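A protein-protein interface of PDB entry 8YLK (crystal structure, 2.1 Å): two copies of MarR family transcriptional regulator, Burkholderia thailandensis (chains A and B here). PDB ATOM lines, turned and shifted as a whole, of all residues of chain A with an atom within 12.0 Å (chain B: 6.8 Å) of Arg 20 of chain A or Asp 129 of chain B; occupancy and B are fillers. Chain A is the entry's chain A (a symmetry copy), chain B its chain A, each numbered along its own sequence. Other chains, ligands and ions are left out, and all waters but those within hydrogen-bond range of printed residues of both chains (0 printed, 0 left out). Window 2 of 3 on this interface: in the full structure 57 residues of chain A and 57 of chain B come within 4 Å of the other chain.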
ATOM      1  N   HIS A  11      22.774 -23.492  32.266  1.00  0.00           N
ATOM      2  CA  HIS A  11      23.069 -24.446  31.205  1.00  0.00           C
ATOM      3  C   HIS A  11      22.177 -24.207  29.994  1.00  0.00           C
ATOM      4  O   HIS A  11      22.635 -24.295  28.848  1.00  0.00           O
ATOM      5  CB  HIS A  11      22.902 -25.872  31.727  1.00  0.00           C
ATOM      6  CG  HIS A  11      23.174 -26.927  30.702  1.00  0.00           C
ATOM      7  ND1 HIS A  11      24.373 -27.021  30.031  1.00  0.00           N
ATOM      8  CD2 HIS A  11      22.399 -27.935  30.234  1.00  0.00           C
ATOM      9  CE1 HIS A  11      24.327 -28.042  29.193  1.00  0.00           C
ATOM     10  NE2 HIS A  11      23.141 -28.614  29.297  1.00  0.00           N
ATOM     11  N   ALA A  12      20.901 -23.895  30.231  1.00  0.00           N
ATOM     12  CA  ALA A  12      19.982 -23.628  29.129  1.00  0.00           C
ATOM     13  C   ALA A  12      20.402 -22.384  28.352  1.00  0.00           C
ATOM     14  O   ALA A  12      20.457 -22.401  27.118  1.00  0.00           O
ATOM     15  CB  ALA A  12      18.558 -23.482  29.662  1.00  0.00           C
ATOM     16  N   VAL A  13      20.701 -21.293  29.064  1.00  0.00           N
ATOM     17  CA  VAL A  13      21.147 -20.068  28.405  1.00  0.00           C
ATOM     18  C   VAL A  13      22.447 -20.309  27.653  1.00  0.00           C
ATOM     19  O   VAL A  13      22.650 -19.793  26.547  1.00  0.00           O
ATOM     20  CB  VAL A  13      21.282 -18.928  29.434  1.00  0.00           C
ATOM     21  CG1 VAL A  13      22.214 -17.838  28.916  1.00  0.00           C
ATOM     22  CG2 VAL A  13      19.919 -18.342  29.745  1.00  0.00           C
ATOM     23  N   GLU A  14      23.343 -21.107  28.234  1.00  0.00           N
ATOM     24  CA  GLU A  14      24.580 -21.458  27.546  1.00  0.00           C
ATOM     25  C   GLU A  14      24.295 -22.155  26.223  1.00  0.00           C
ATOM     26  O   GLU A  14      24.960 -21.889  25.216  1.00  0.00           O
ATOM     27  CB  GLU A  14      25.442 -22.347  28.444  1.00  0.00           C
ATOM     28  CG  GLU A  14      26.790 -22.718  27.850  1.00  0.00           C
ATOM     29  CD  GLU A  14      27.811 -21.608  27.996  1.00  0.00           C
ATOM     30  OE1 GLU A  14      27.581 -20.701  28.821  1.00  0.00           O
ATOM     31  OE2 GLU A  14      28.842 -21.644  27.289  1.00  0.00           O
ATOM     32  N   GLN A  15      23.307 -23.051  26.203  1.00  0.00           N
ATOM     33  CA  GLN A  15      23.000 -23.772  24.974  1.00  0.00           C
ATOM     34  C   GLN A  15      22.378 -22.848  23.935  1.00  0.00           C
ATOM     35  O   GLN A  15      22.653 -22.983  22.736  1.00  0.00           O
ATOM     36  CB  GLN A  15      22.074 -24.952  25.273  1.00  0.00           C
ATOM     37  CG  GLN A  15      22.749 -26.096  26.018  1.00  0.00           C
ATOM     38  CD  GLN A  15      21.844 -27.301  26.172  1.00  0.00           C
ATOM     39  OE1 GLN A  15      20.641 -27.167  26.400  1.00  0.00           O
ATOM     40  NE2 GLN A  15      22.417 -28.488  26.035  1.00  0.00           N
ATOM     41  N   TRP A  16      21.547 -21.901  24.378  1.00  0.00           N
ATOM     42  CA  TRP A  16      20.893 -20.985  23.447  1.00  0.00           C
ATOM     43  C   TRP A  16      21.903 -20.084  22.752  1.00  0.00           C
ATOM     44  O   TRP A  16      21.828 -19.878  21.536  1.00  0.00           O
ATOM     45  CB  TRP A  16      19.842 -20.150  24.178  1.00  0.00           C
ATOM     46  CG  TRP A  16      18.523 -20.839  24.319  1.00  0.00           C
ATOM     47  CD1 TRP A  16      17.874 -21.130  25.477  1.00  0.00           C
ATOM     48  CD2 TRP A  16      17.693 -21.327  23.258  1.00  0.00           C
ATOM     49  NE1 TRP A  16      16.685 -21.767  25.207  1.00  0.00           N
ATOM     50  CE2 TRP A  16      16.552 -21.899  23.849  1.00  0.00           C
ATOM     51  CE3 TRP A  16      17.803 -21.330  21.863  1.00  0.00           C
ATOM     52  CZ2 TRP A  16      15.529 -22.474  23.099  1.00  0.00           C
ATOM     53  CZ3 TRP A  16      16.785 -21.901  21.118  1.00  0.00           C
ATOM     54  CH2 TRP A  16      15.663 -22.464  21.738  1.00  0.00           C
ATOM     55  N   ARG A  17      22.851 -19.525  23.511  1.00  0.00           N
ATOM     56  CA  ARG A  17      23.871 -18.675  22.905  1.00  0.00           C
ATOM     57  C   ARG A  17      24.660 -19.421  21.838  1.00  0.00           C
ATOM     58  O   ARG A  17      25.164 -18.804  20.891  1.00  0.00           O
ATOM     59  CB  ARG A  17      24.803 -18.121  23.985  1.00  0.00           C
ATOM     60  CG  ARG A  17      24.192 -16.966  24.766  1.00  0.00           C
ATOM     61  CD  ARG A  17      24.986 -16.607  26.013  1.00  0.00           C
ATOM     62  NE  ARG A  17      24.330 -15.531  26.753  1.00  0.00           N
ATOM     63  CZ  ARG A  17      24.680 -15.130  27.971  1.00  0.00           C
ATOM     64  NH1 ARG A  17      25.687 -15.715  28.605  1.00  0.00           N
ATOM     65  NH2 ARG A  17      24.014 -14.145  28.559  1.00  0.00           N
ATOM     66  N   SER A  18      24.756 -20.746  21.958  1.00  0.00           N
ATOM     67  CA  SER A  18      25.435 -21.544  20.944  1.00  0.00           C
ATOM     68  C   SER A  18      24.527 -21.852  19.755  1.00  0.00           C
ATOM     69  O   SER A  18      24.979 -21.819  18.605  1.00  0.00           O
ATOM     70  CB  SER A  18      25.955 -22.839  21.569  1.00  0.00           C
ATOM     71  OG  SER A  18      26.318 -23.774  20.570  1.00  0.00           O
ATOM     72  N   GLU A  19      23.250 -22.148  20.008  1.00  0.00           N
ATOM     73  CA  GLU A  19      22.345 -22.584  18.946  1.00  0.00           C
ATOM     74  C   GLU A  19      21.623 -21.435  18.250  1.00  0.00           C
ATOM     75  O   GLU A  19      21.343 -21.530  17.048  1.00  0.00           O
ATOM     76  CB  GLU A  19      21.316 -23.574  19.506  1.00  0.00           C
ATOM     77  CG  GLU A  19      21.863 -24.976  19.720  1.00  0.00           C
ATOM     78  CD  GLU A  19      22.135 -25.698  18.412  1.00  0.00           C
ATOM     79  OE1 GLU A  19      21.377 -25.478  17.442  1.00  0.00           O
ATOM     80  OE2 GLU A  19      23.107 -26.483  18.355  1.00  0.00           O
ATOM     81  N   ARG A  20      21.306 -20.357  18.967  1.00  0.00           N
ATOM     82  CA  ARG A  20      20.602 -19.203  18.405  1.00  0.00           C
ATOM     83  C   ARG A  20      21.330 -17.925  18.803  1.00  0.00           C
ATOM     84  O   ARG A  20      20.839 -17.147  19.631  1.00  0.00           O
ATOM     85  CB  ARG A  20      19.146 -19.165  18.873  1.00  0.00           C
ATOM     86  CG  ARG A  20      18.270 -20.284  18.332  1.00  0.00           C
ATOM     87  CD  ARG A  20      17.964 -20.087  16.859  1.00  0.00           C
ATOM     88  NE  ARG A  20      17.488 -18.734  16.585  1.00  0.00           N
ATOM     89  CZ  ARG A  20      16.210 -18.366  16.602  1.00  0.00           C
ATOM     90  NH1 ARG A  20      15.259 -19.251  16.876  1.00  0.00           N
ATOM     91  NH2 ARG A  20      15.884 -17.106  16.341  1.00  0.00           N
ATOM     92  N   PRO A  21      22.504 -17.668  18.218  1.00  0.00           N
ATOM     93  CA  PRO A  21      23.259 -16.462  18.593  1.00  0.00           C
ATOM     94  C   PRO A  21      22.560 -15.166  18.225  1.00  0.00           C
ATOM     95  O   PRO A  21      22.953 -14.107  18.732  1.00  0.00           O
ATOM     96  CB  PRO A  21      24.577 -16.621  17.828  1.00  0.00           C
ATOM     97  CG  PRO A  21      24.224 -17.471  16.658  1.00  0.00           C
ATOM     98  CD  PRO A  21      23.180 -18.432  17.155  1.00  0.00           C
ATOM     99  N   ASP A  22      21.544 -15.208  17.361  1.00  0.00           N
ATOM    100  CA  ASP A  22      20.742 -14.025  17.077  1.00  0.00           C
ATOM    101  C   ASP A  22      19.871 -13.607  18.256  1.00  0.00           C
ATOM    102  O   ASP A  22      19.289 -12.516  18.213  1.00  0.00           O
ATOM    103  CB  ASP A  22      19.860 -14.276  15.854  1.00  0.00           C
ATOM    104  CG  ASP A  22      19.069 -15.564  15.964  1.00  0.00           C
ATOM    105  OD1 ASP A  22      19.689 -16.624  16.186  1.00  0.00           O
ATOM    106  OD2 ASP A  22      17.827 -15.517  15.843  1.00  0.00           O
ATOM    107  N   LEU A  23      19.777 -14.435  19.295  1.00  0.00           N
ATOM    108  CA  LEU A  23      18.925 -14.199  20.452  1.00  0.00           C
ATOM    109  C   LEU A  23      19.712 -13.606  21.612  1.00  0.00           C
ATOM    110  O   LEU A  23      20.917 -13.831  21.755  1.00  0.00           O
ATOM    111  CB  LEU A  23      18.270 -15.501  20.921  1.00  0.00           C
ATOM    112  CG  LEU A  23      16.958 -15.947  20.284  1.00  0.00           C
ATOM    113  CD1 LEU A  23      16.421 -17.164  21.016  1.00  0.00           C
ATOM    114  CD2 LEU A  23      15.951 -14.814  20.311  1.00  0.00           C
ATOM    115  N   ASP A  24      19.005 -12.861  22.461  1.00  0.00           N
ATOM    116  CA  ASP A  24      19.531 -12.376  23.733  1.00  0.00           C
ATOM    117  C   ASP A  24      18.807 -13.119  24.849  1.00  0.00           C
ATOM    118  O   ASP A  24      17.752 -12.669  25.323  1.00  0.00           O
ATOM    119  CB  ASP A  24      19.341 -10.864  23.867  1.00  0.00           C
ATOM    120  CG  ASP A  24      19.704 -10.352  25.242  1.00  0.00           C
ATOM    121  OD1 ASP A  24      20.790 -10.711  25.738  1.00  0.00           O
ATOM    122  OD2 ASP A  24      18.904  -9.593  25.826  1.00  0.00           O
ATOM    123  N   PRO A  25      19.322 -14.268  25.297  1.00  0.00           N
ATOM    124  CA  PRO A  25      18.570 -15.092  26.253  1.00  0.00           C
ATOM    125  C   PRO A  25      18.852 -14.756  27.708  1.00  0.00           C
ATOM    126  O   PRO A  25      18.593 -15.579  28.589  1.00  0.00           O
ATOM    127  CB  PRO A  25      19.044 -16.510  25.920  1.00  0.00           C
ATOM    128  CG  PRO A  25      20.477 -16.307  25.509  1.00  0.00           C
ATOM    129  CD  PRO A  25      20.546 -14.944  24.830  1.00  0.00           C
ATOM    130  N   SER A  26      19.373 -13.556  27.974  1.00  0.00           N
ATOM    131  CA  SER A  26      19.795 -13.215  29.330  1.00  0.00           C
ATOM    132  C   SER A  26      18.638 -13.310  30.322  1.00  0.00           C
ATOM    133  O   SER A  26      18.817 -13.785  31.452  1.00  0.00           O
ATOM    134  CB  SER A  26      20.417 -11.816  29.349  1.00  0.00           C
ATOM    135  OG  SER A  26      19.735 -10.936  28.474  1.00  0.00           O
ATOM    136  N   SER A  27      17.439 -12.900  29.907  1.00  0.00           N
ATOM    137  CA  SER A  27      16.294 -12.877  30.811  1.00  0.00           C
ATOM    138  C   SER A  27      15.868 -14.266  31.272  1.00  0.00           C
ATOM    139  O   SER A  27      15.107 -14.377  32.240  1.00  0.00           O
ATOM    140  CB  SER A  27      15.117 -12.190  30.129  1.00  0.00           C
ATOM    141  OG  SER A  27      14.704 -12.937  28.999  1.00  0.00           O
ATOM    142  N   MET A  28      16.339 -15.325  30.609  1.00  0.00           N
ATOM    143  CA  MET A  28      15.906 -16.673  30.967  1.00  0.00           C
ATOM    144  C   MET A  28      16.402 -17.095  32.344  1.00  0.00           C
ATOM    145  O   MET A  28      15.725 -17.868  33.031  1.00  0.00           O
ATOM    146  CB  MET A  28      16.385 -17.678  29.924  1.00  0.00           C
ATOM    147  CG  MET A  28      15.747 -17.543  28.559  1.00  0.00           C
ATOM    148  SD  MET A  28      16.474 -18.733  27.421  1.00  0.00           S
ATOM    149  CE  MET A  28      15.339 -18.644  26.039  1.00  0.00           C
ATOM    150  N   ARG B  67      15.278 -28.216  21.096  1.00  0.00           N
ATOM    151  CA  ARG B  67      15.900 -27.328  20.121  1.00  0.00           C
ATOM    152  C   ARG B  67      17.318 -26.964  20.538  1.00  0.00           C
ATOM    153  O   ARG B  67      18.268 -27.121  19.760  1.00  0.00           O
ATOM    154  CB  ARG B  67      15.051 -26.072  19.945  1.00  0.00           C
ATOM    155  CG  ARG B  67      15.674 -25.036  19.028  1.00  0.00           C
ATOM    156  CD  ARG B  67      15.801 -25.548  17.601  1.00  0.00           C
ATOM    157  NE  ARG B  67      16.468 -24.574  16.736  1.00  0.00           N
ATOM    158  CZ  ARG B  67      17.786 -24.412  16.687  1.00  0.00           C
ATOM    159  NH1 ARG B  67      18.573 -25.154  17.459  1.00  0.00           N
ATOM    160  NH2 ARG B  67      18.317 -23.509  15.880  1.00  0.00           N
ATOM    161  N   TYR B  73      18.286 -32.645  17.176  1.00  0.00           N
ATOM    162  CA  TYR B  73      17.247 -32.241  18.125  1.00  0.00           C
ATOM    163  C   TYR B  73      16.492 -33.456  18.663  1.00  0.00           C
ATOM    164  O   TYR B  73      15.260 -33.503  18.664  1.00  0.00           O
ATOM    165  CB  TYR B  73      16.287 -31.227  17.489  1.00  0.00           C
ATOM    166  CG  TYR B  73      16.975 -30.199  16.613  1.00  0.00           C
ATOM    167  CD1 TYR B  73      17.694 -29.146  17.168  1.00  0.00           C
ATOM    168  CD2 TYR B  73      16.908 -30.283  15.230  1.00  0.00           C
ATOM    169  CE1 TYR B  73      18.328 -28.207  16.365  1.00  0.00           C
ATOM    170  CE2 TYR B  73      17.538 -29.352  14.422  1.00  0.00           C
ATOM    171  CZ  TYR B  73      18.246 -28.317  14.993  1.00  0.00           C
ATOM    172  OH  TYR B  73      18.872 -27.393  14.180  1.00  0.00           O
ATOM    173  N   GLY B 124       7.709 -28.878  14.411  1.00  0.00           N
ATOM    174  CA  GLY B 124       8.054 -28.547  15.781  1.00  0.00           C
ATOM    175  C   GLY B 124       9.265 -27.642  15.875  1.00  0.00           C
ATOM    176  O   GLY B 124       9.290 -26.707  16.677  1.00  0.00           O
ATOM    177  N   ARG B 125      10.291 -27.913  15.067  1.00  0.00           N
ATOM    178  CA  ARG B 125      11.474 -27.062  15.075  1.00  0.00           C
ATOM    179  C   ARG B 125      11.117 -25.633  14.672  1.00  0.00           C
ATOM    180  O   ARG B 125      11.511 -24.668  15.337  1.00  0.00           O
ATOM    181  CB  ARG B 125      12.536 -27.648  14.144  1.00  0.00           C
ATOM    182  CG  ARG B 125      13.872 -26.920  14.154  1.00  0.00           C
ATOM    183  CD  ARG B 125      14.136 -26.268  12.814  1.00  0.00           C
ATOM    184  NE  ARG B 125      15.450 -25.634  12.739  1.00  0.00           N
ATOM    185  CZ  ARG B 125      16.442 -26.057  11.960  1.00  0.00           C
ATOM    186  NH1 ARG B 125      16.274 -27.121  11.184  1.00  0.00           N
ATOM    187  NH2 ARG B 125      17.601 -25.412  11.951  1.00  0.00           N
ATOM    188  N   ALA B 126      10.350 -25.481  13.591  1.00  0.00           N
ATOM    189  CA  ALA B 126       9.952 -24.148  13.152  1.00  0.00           C
ATOM    190  C   ALA B 126       9.114 -23.441  14.212  1.00  0.00           C
ATOM    191  O   ALA B 126       9.288 -22.239  14.449  1.00  0.00           O
ATOM    192  CB  ALA B 126       9.184 -24.234  11.836  1.00  0.00           C
ATOM    193  N   LEU B 127       8.204 -24.172  14.861  1.00  0.00           N
ATOM    194  CA  LEU B 127       7.366 -23.565  15.891  1.00  0.00           C
ATOM    195  C   LEU B 127       8.213 -22.992  17.019  1.00  0.00           C
ATOM    196  O   LEU B 127       8.038 -21.835  17.418  1.00  0.00           O
ATOM    197  CB  LEU B 127       6.366 -24.587  16.435  1.00  0.00           C
ATOM    198  CG  LEU B 127       5.547 -24.156  17.656  1.00  0.00           C
ATOM    199  CD1 LEU B 127       4.641 -22.981  17.339  1.00  0.00           C
ATOM    200  CD2 LEU B 127       4.732 -25.309  18.187  1.00  0.00           C
ATOM    201  N   ILE B 128       9.157 -23.783  17.536  1.00  0.00           N
ATOM    202  CA  ILE B 128       9.940 -23.312  18.673  1.00  0.00           C
ATOM    203  C   ILE B 128      10.922 -22.228  18.243  1.00  0.00           C
ATOM    204  O   ILE B 128      11.214 -21.309  19.020  1.00  0.00           O
ATOM    205  CB  ILE B 128      10.646 -24.487  19.381  1.00  0.00           C
ATOM    206  CG1 ILE B 128      11.302 -24.001  20.672  1.00  0.00           C
ATOM    207  CG2 ILE B 128      11.686 -25.145  18.478  1.00  0.00           C
ATOM    208  CD1 ILE B 128      10.331 -23.354  21.623  1.00  0.00           C
ATOM    209  N   ASP B 129      11.441 -22.304  17.012  1.00  0.00           N
ATOM    210  CA  ASP B 129      12.311 -21.241  16.516  1.00  0.00           C
ATOM    211  C   ASP B 129      11.575 -19.909  16.490  1.00  0.00           C
ATOM    212  O   ASP B 129      12.160 -18.858  16.776  1.00  0.00           O
ATOM    213  CB  ASP B 129      12.834 -21.586  15.118  1.00  0.00           C
ATOM    214  CG  ASP B 129      14.149 -22.352  15.149  1.00  0.00           C
ATOM    215  OD1 ASP B 129      14.854 -22.297  16.178  1.00  0.00           O
ATOM    216  OD2 ASP B 129      14.481 -22.995  14.130  1.00  0.00           O
ATOM    217  N   ASP B 130      10.284 -19.941  16.157  1.00  0.00           N
ATOM    218  CA  ASP B 130       9.467 -18.733  16.162  1.00  0.00           C
ATOM    219  C   ASP B 130       9.094 -18.330  17.585  1.00  0.00           C
ATOM    220  O   ASP B 130       9.195 -17.155  17.958  1.00  0.00           O
ATOM    221  CB  ASP B 130       8.214 -18.969  15.320  1.00  0.00           C
ATOM    222  CG  ASP B 130       7.520 -17.681  14.919  1.00  0.00           C
ATOM    223  OD1 ASP B 130       8.006 -16.588  15.285  1.00  0.00           O
ATOM    224  OD2 ASP B 130       6.482 -17.773  14.233  1.00  0.00           O
ATOM    225  N   ALA B 131       8.680 -19.304  18.402  1.00  0.00           N
ATOM    226  CA  ALA B 131       8.154 -18.990  19.726  1.00  0.00           C
ATOM    227  C   ALA B 131       9.230 -18.416  20.638  1.00  0.00           C
ATOM    228  O   ALA B 131       8.957 -17.504  21.429  1.00  0.00           O
ATOM    229  CB  ALA B 131       7.539 -20.240  20.358  1.00  0.00           C
ATOM    230  N   VAL B 132      10.455 -18.939  20.553  1.00  0.00           N
ATOM    231  CA  VAL B 132      11.480 -18.534  21.509  1.00  0.00           C
ATOM    232  C   VAL B 132      11.840 -17.062  21.326  1.00  0.00           C
ATOM    233  O   VAL B 132      12.141 -16.367  22.304  1.00  0.00           O
ATOM    234  CB  VAL B 132      12.711 -19.454  21.401  1.00  0.00           C
ATOM    235  CG1 VAL B 132      13.456 -19.229  20.102  1.00  0.00           C
ATOM    236  CG2 VAL B 132      13.630 -19.251  22.600  1.00  0.00           C
ATOM    237  N   VAL B 133      11.792 -16.554  20.093  1.00  0.00           N
ATOM    238  CA  VAL B 133      12.018 -15.128  19.876  1.00  0.00           C
ATOM    239  C   VAL B 133      10.958 -14.309  20.603  1.00  0.00           C
ATOM    240  O   VAL B 133      11.273 -13.375  21.353  1.00  0.00           O
ATOM    241  CB  VAL B 133      12.048 -14.805  18.372  1.00  0.00           C
ATOM    242  CG1 VAL B 133      12.017 -13.301  18.158  1.00  0.00           C
ATOM    243  CG2 VAL B 133      13.289 -15.397  17.726  1.00  0.00           C
ATOM    244  N   ALA B 134       9.684 -14.645  20.397  1.00  0.00           N
ATOM    245  CA  ALA B 134       8.632 -13.901  21.081  1.00  0.00           C
ATOM    246  C   ALA B 134       8.697 -14.118  22.583  1.00  0.00           C
ATOM    247  O   ALA B 134       8.321 -13.231  23.358  1.00  0.00           O
ATOM    248  CB  ALA B 134       7.258 -14.295  20.537  1.00  0.00           C
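The side-chain carboxylate of Asp 129 of chain B lies within salt-bridge range of the guanidinium group of Arg 20 of chain A (3.2 Å). The guanidinium group of Arg 67 of chain B lies within salt-bridge range of the side-chain carboxylate of Glu 19 of chain A, 2.8 Å away.
The indole nitrogen of Trp 16 of chain A lies close to the side-chain sulfur of Met 28 of chain A, at 3.8 Å. OD2 of Asp 129 of chain B lies within salt-bridge range of NE of Arg 125 of chain B, 3.1 Å away. The side-chain carboxylate of Asp 129 of chain B lies within salt-bridge range of the guanidinium group of Arg 67 of chain B (2.8 Å). NH2 of Arg 20 of chain A is in salt-bridge range of OD2 of Asp 22 of chain A.
Among the printed residues, pairs that only touch across the chains: Trp 16 of chain A with Arg 67 of chain B, Trp 16 of chain A with Val 132 of chain B, Arg 20 of chain A with Arg 67 of chain B, Arg 20 of chain A with Val 132 of chain B, Arg 20 of chain A with Val 133 of chain B, Leu 23 of chain A with Val 132 of chain B, Leu 23 of chain A with Val 133 of chain B and Met 28 of chain A with Val 132 of chain B.
Of chain B, only Arg 67, Asp 129, Val 132 and Val 133 come within 4 Å of Arg 20 of chain A. Of chain A, only Trp 16, Glu 19 and Arg 20 come within 4 Å of Arg 67 of chain B. Arg 125 of chain B touches none of the printed residues of chain A. No residue of chain A comes within 4 Å of Ala 126 of chain B. No residue of chain A comes within 4 Å of Ile 128 of chain B. No residue of chain A comes within 4 Å of Ala 131 of chain B. Of chain A, only Trp 16, Arg 20, Leu 23 and Met 28 come within 4 Å of Val 132 of chain B. Of the printed residues of chain B, Leu 23 of chain A touches Val 132 (3.7 Å) and Val 133 (3.8 Å). Of the printed residues of chain B, Glu 19 of chain A touches Arg 67 (2.8 Å). Printed residues of chain B within 4 Å of Met 28 of chain A: Val 132 (3.9 Å). Val 13 of chain A touches none of the printed residues of chain B. Pro 25 of chain A touches none of the printed residues of chain B. The nearest residue of chain B that does not touch Arg 20 of chain A is Ile 128 of chain B (5.0 Å). The nearest residue of chain A that does not touch Asp 129 of chain B is Trp 16 of chain A (5.3 Å). The nearest printed residue of chain B that does not touch Trp 16 of chain A is Ile 128 of chain B (4.7 Å).
Printed residues of chain A that touch a printed residue of chain B: Trp 16, Glu 19, Arg 20, Leu 23 and Met 28. Hydrophobic or aromatic side chains of chain A within 4 Å of the printed part of chain B: Trp 16, Leu 23 and Met 28. Hydrophobic or aromatic side chains of chain B within 4 Å of the printed part of chain A: Val 132 and Val 133.
No position is printed for both chains.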
